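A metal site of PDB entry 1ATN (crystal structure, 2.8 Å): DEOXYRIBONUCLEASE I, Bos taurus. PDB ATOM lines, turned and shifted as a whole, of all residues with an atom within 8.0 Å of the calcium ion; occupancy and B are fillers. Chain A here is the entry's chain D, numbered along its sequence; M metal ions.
OG1 of Thr 205 is in hydrogen-bond range of OG1 of Thr 207 (3.0 Å).
The backbone carbonyl oxygen of Thr 203 sits close to the side-chain hydroxyl of Tyr 253, 3.5 Å away.
Along chain A the residues within 4 Å of the calcium ion span positions 201 to 207.
The calcium ion is bound by OD2 of Asp 201 (2.3 Å).
The calcium ion is bound by OD1 of Asp 201 (2.5 Å).
O of Thr 205 is bound to the calcium ion, at 2.5 Å.
O of Thr 203 binds the calcium ion, at 2.7 Å.
The calcium ion is bound by O of Thr 207, at 2.7 Å.
The calcium ion is bound by OG1 of Thr 203, at 2.7 Å.
The calcium ion has six donor atoms within binding distance.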
ATOM      1  N   ALA A 200      22.916  29.574  -3.151  1.00  0.00           N
ATOM      2  CA  ALA A 200      22.983  28.193  -3.597  1.00  0.00           C
ATOM      3  C   ALA A 200      23.149  27.953  -5.097  1.00  0.00           C
ATOM      4  O   ALA A 200      22.655  28.698  -5.948  1.00  0.00           O
ATOM      5  CB  ALA A 200      21.740  27.514  -3.059  1.00  0.00           C
ATOM      6  N   ASP A 201      24.043  27.010  -5.350  1.00  0.00           N
ATOM      7  CA  ASP A 201      24.428  26.476  -6.644  1.00  0.00           C
ATOM      8  C   ASP A 201      23.544  25.266  -6.675  1.00  0.00           C
ATOM      9  O   ASP A 201      23.613  24.489  -5.729  1.00  0.00           O
ATOM     10  CB  ASP A 201      25.861  26.009  -6.652  1.00  0.00           C
ATOM     11  CG  ASP A 201      26.431  25.435  -7.945  1.00  0.00           C
ATOM     12  OD1 ASP A 201      25.881  25.572  -9.014  1.00  0.00           O
ATOM     13  OD2 ASP A 201      27.480  24.829  -7.911  1.00  0.00           O
ATOM     14  N   THR A 202      22.696  25.027  -7.634  1.00  0.00           N
ATOM     15  CA  THR A 202      21.941  23.816  -7.603  1.00  0.00           C
ATOM     16  C   THR A 202      22.187  23.223  -8.962  1.00  0.00           C
ATOM     17  O   THR A 202      21.402  22.365  -9.344  1.00  0.00           O
ATOM     18  CB  THR A 202      20.410  24.048  -7.403  1.00  0.00           C
ATOM     19  OG1 THR A 202      20.053  24.862  -8.489  1.00  0.00           O
ATOM     20  CG2 THR A 202      19.969  24.697  -6.105  1.00  0.00           C
ATOM     21  N   THR A 203      23.206  23.637  -9.736  1.00  0.00           N
ATOM     22  CA  THR A 203      23.507  23.002 -10.996  1.00  0.00           C
ATOM     23  C   THR A 203      24.615  21.984 -10.849  1.00  0.00           C
ATOM     24  O   THR A 203      25.547  22.256 -10.083  1.00  0.00           O
ATOM     25  CB  THR A 203      24.018  23.925 -12.083  1.00  0.00           C
ATOM     26  OG1 THR A 203      25.232  24.513 -11.625  1.00  0.00           O
ATOM     27  CG2 THR A 203      22.985  24.967 -12.434  1.00  0.00           C
ATOM     28  N   ALA A 204      24.554  20.841 -11.548  1.00  0.00           N
ATOM     29  CA  ALA A 204      25.669  19.936 -11.579  1.00  0.00           C
ATOM     30  C   ALA A 204      26.774  20.428 -12.499  1.00  0.00           C
ATOM     31  O   ALA A 204      27.912  19.950 -12.343  1.00  0.00           O
ATOM     32  CB  ALA A 204      25.293  18.553 -12.079  1.00  0.00           C
ATOM     33  N   THR A 205      26.495  21.354 -13.442  1.00  0.00           N
ATOM     34  CA  THR A 205      27.520  21.911 -14.313  1.00  0.00           C
ATOM     35  C   THR A 205      28.264  23.057 -13.634  1.00  0.00           C
ATOM     36  O   THR A 205      27.875  23.616 -12.590  1.00  0.00           O
ATOM     37  CB  THR A 205      26.912  22.468 -15.613  1.00  0.00           C
ATOM     38  OG1 THR A 205      26.127  23.595 -15.242  1.00  0.00           O
ATOM     39  CG2 THR A 205      26.044  21.464 -16.357  1.00  0.00           C
ATOM     40  N   SER A 206      29.357  23.470 -14.278  1.00  0.00           N
ATOM     41  CA  SER A 206      30.220  24.600 -13.888  1.00  0.00           C
ATOM     42  C   SER A 206      29.613  25.957 -13.416  1.00  0.00           C
ATOM     43  O   SER A 206      30.244  26.659 -12.608  1.00  0.00           O
ATOM     44  CB  SER A 206      31.162  24.790 -15.082  1.00  0.00           C
ATOM     45  OG  SER A 206      30.546  24.408 -16.324  1.00  0.00           O
ATOM     46  N   THR A 207      28.405  26.320 -13.924  1.00  0.00           N
ATOM     47  CA  THR A 207      27.620  27.488 -13.559  1.00  0.00           C
ATOM     48  C   THR A 207      27.268  27.449 -12.069  1.00  0.00           C
ATOM     49  O   THR A 207      27.274  26.370 -11.471  1.00  0.00           O
ATOM     50  CB  THR A 207      26.339  27.485 -14.356  1.00  0.00           C
ATOM     51  OG1 THR A 207      25.562  26.318 -14.053  1.00  0.00           O
ATOM     52  CG2 THR A 207      26.679  27.425 -15.833  1.00  0.00           C
ATOM     53  N   ASN A 208      26.976  28.608 -11.462  1.00  0.00           N
ATOM     54  CA  ASN A 208      26.480  28.720 -10.096  1.00  0.00           C
ATOM     55  C   ASN A 208      25.193  29.557 -10.097  1.00  0.00           C
ATOM     56  O   ASN A 208      25.117  30.816 -10.121  1.00  0.00           O
ATOM     57  CB  ASN A 208      27.408  29.430  -9.090  1.00  0.00           C
ATOM     58  CG  ASN A 208      26.781  29.698  -7.698  1.00  0.00           C
ATOM     59  OD1 ASN A 208      25.673  30.242  -7.473  1.00  0.00           O
ATOM     60  ND2 ASN A 208      27.549  29.269  -6.700  1.00  0.00           N
ATOM     61  N   CYS A 209      24.139  28.778  -9.908  1.00  0.00           N
ATOM     62  CA  CYS A 209      22.808  29.355  -9.919  1.00  0.00           C
ATOM     63  C   CYS A 209      21.906  28.593  -8.983  1.00  0.00           C
ATOM     64  O   CYS A 209      22.086  27.402  -8.789  1.00  0.00           O
ATOM     65  CB  CYS A 209      22.340  29.304 -11.322  1.00  0.00           C
ATOM     66  SG  CYS A 209      23.517  30.008 -12.523  1.00  0.00           S
ATOM     67  N   ASP A 234      24.435  17.459  -3.330  1.00  0.00           N
ATOM     68  CA  ASP A 234      25.557  17.225  -4.179  1.00  0.00           C
ATOM     69  C   ASP A 234      25.919  15.770  -4.339  1.00  0.00           C
ATOM     70  O   ASP A 234      26.830  15.300  -3.713  1.00  0.00           O
ATOM     71  CB  ASP A 234      26.769  17.985  -3.656  1.00  0.00           C
ATOM     72  CG  ASP A 234      27.700  18.229  -4.853  1.00  0.00           C
ATOM     73  OD1 ASP A 234      27.541  17.630  -5.945  1.00  0.00           O
ATOM     74  OD2 ASP A 234      28.603  19.060  -4.673  1.00  0.00           O
ATOM     75  N   GLN A 236      27.265  14.247  -6.845  1.00  0.00           N
ATOM     76  CA  GLN A 236      28.602  14.061  -7.391  1.00  0.00           C
ATOM     77  C   GLN A 236      29.507  14.077  -6.184  1.00  0.00           C
ATOM     78  O   GLN A 236      30.201  13.098  -5.941  1.00  0.00           O
ATOM     79  CB  GLN A 236      29.088  15.205  -8.292  1.00  0.00           C
ATOM     80  CG  GLN A 236      30.433  14.905  -8.921  1.00  0.00           C
ATOM     81  CD  GLN A 236      31.020  15.912  -9.936  1.00  0.00           C
ATOM     82  OE1 GLN A 236      32.205  15.841 -10.294  1.00  0.00           O
ATOM     83  NE2 GLN A 236      30.282  16.887 -10.490  1.00  0.00           N
ATOM     84  N   ASP A 251      22.105  17.472 -15.060  1.00  0.00           N
ATOM     85  CA  ASP A 251      22.779  18.748 -14.946  1.00  0.00           C
ATOM     86  C   ASP A 251      22.287  19.561 -13.757  1.00  0.00           C
ATOM     87  O   ASP A 251      22.723  20.695 -13.619  1.00  0.00           O
ATOM     88  CB  ASP A 251      22.569  19.562 -16.210  1.00  0.00           C
ATOM     89  CG  ASP A 251      21.172  19.646 -16.813  1.00  0.00           C
ATOM     90  OD1 ASP A 251      20.204  19.101 -16.287  1.00  0.00           O
ATOM     91  OD2 ASP A 251      21.058  20.256 -17.871  1.00  0.00           O
ATOM     92  N   TYR A 253      20.803  19.503  -9.227  1.00  0.00           N
ATOM     93  CA  TYR A 253      20.867  18.637  -8.064  1.00  0.00           C
ATOM     94  C   TYR A 253      19.516  18.646  -7.385  1.00  0.00           C
ATOM     95  O   TYR A 253      18.739  19.573  -7.603  1.00  0.00           O
ATOM     96  CB  TYR A 253      21.787  19.108  -7.007  1.00  0.00           C
ATOM     97  CG  TYR A 253      23.220  19.311  -7.379  1.00  0.00           C
ATOM     98  CD1 TYR A 253      23.925  18.298  -7.988  1.00  0.00           C
ATOM     99  CD2 TYR A 253      23.805  20.516  -7.048  1.00  0.00           C
ATOM    100  CE1 TYR A 253      25.269  18.457  -8.284  1.00  0.00           C
ATOM    101  CE2 TYR A 253      25.149  20.686  -7.335  1.00  0.00           C
ATOM    102  CZ  TYR A 253      25.873  19.659  -7.946  1.00  0.00           C
ATOM    103  OH  TYR A 253      27.221  19.819  -8.220  1.00  0.00           O
HETATM  104 CA    CA M   1      27.485  24.074 -10.115  1.00  0.00          CA
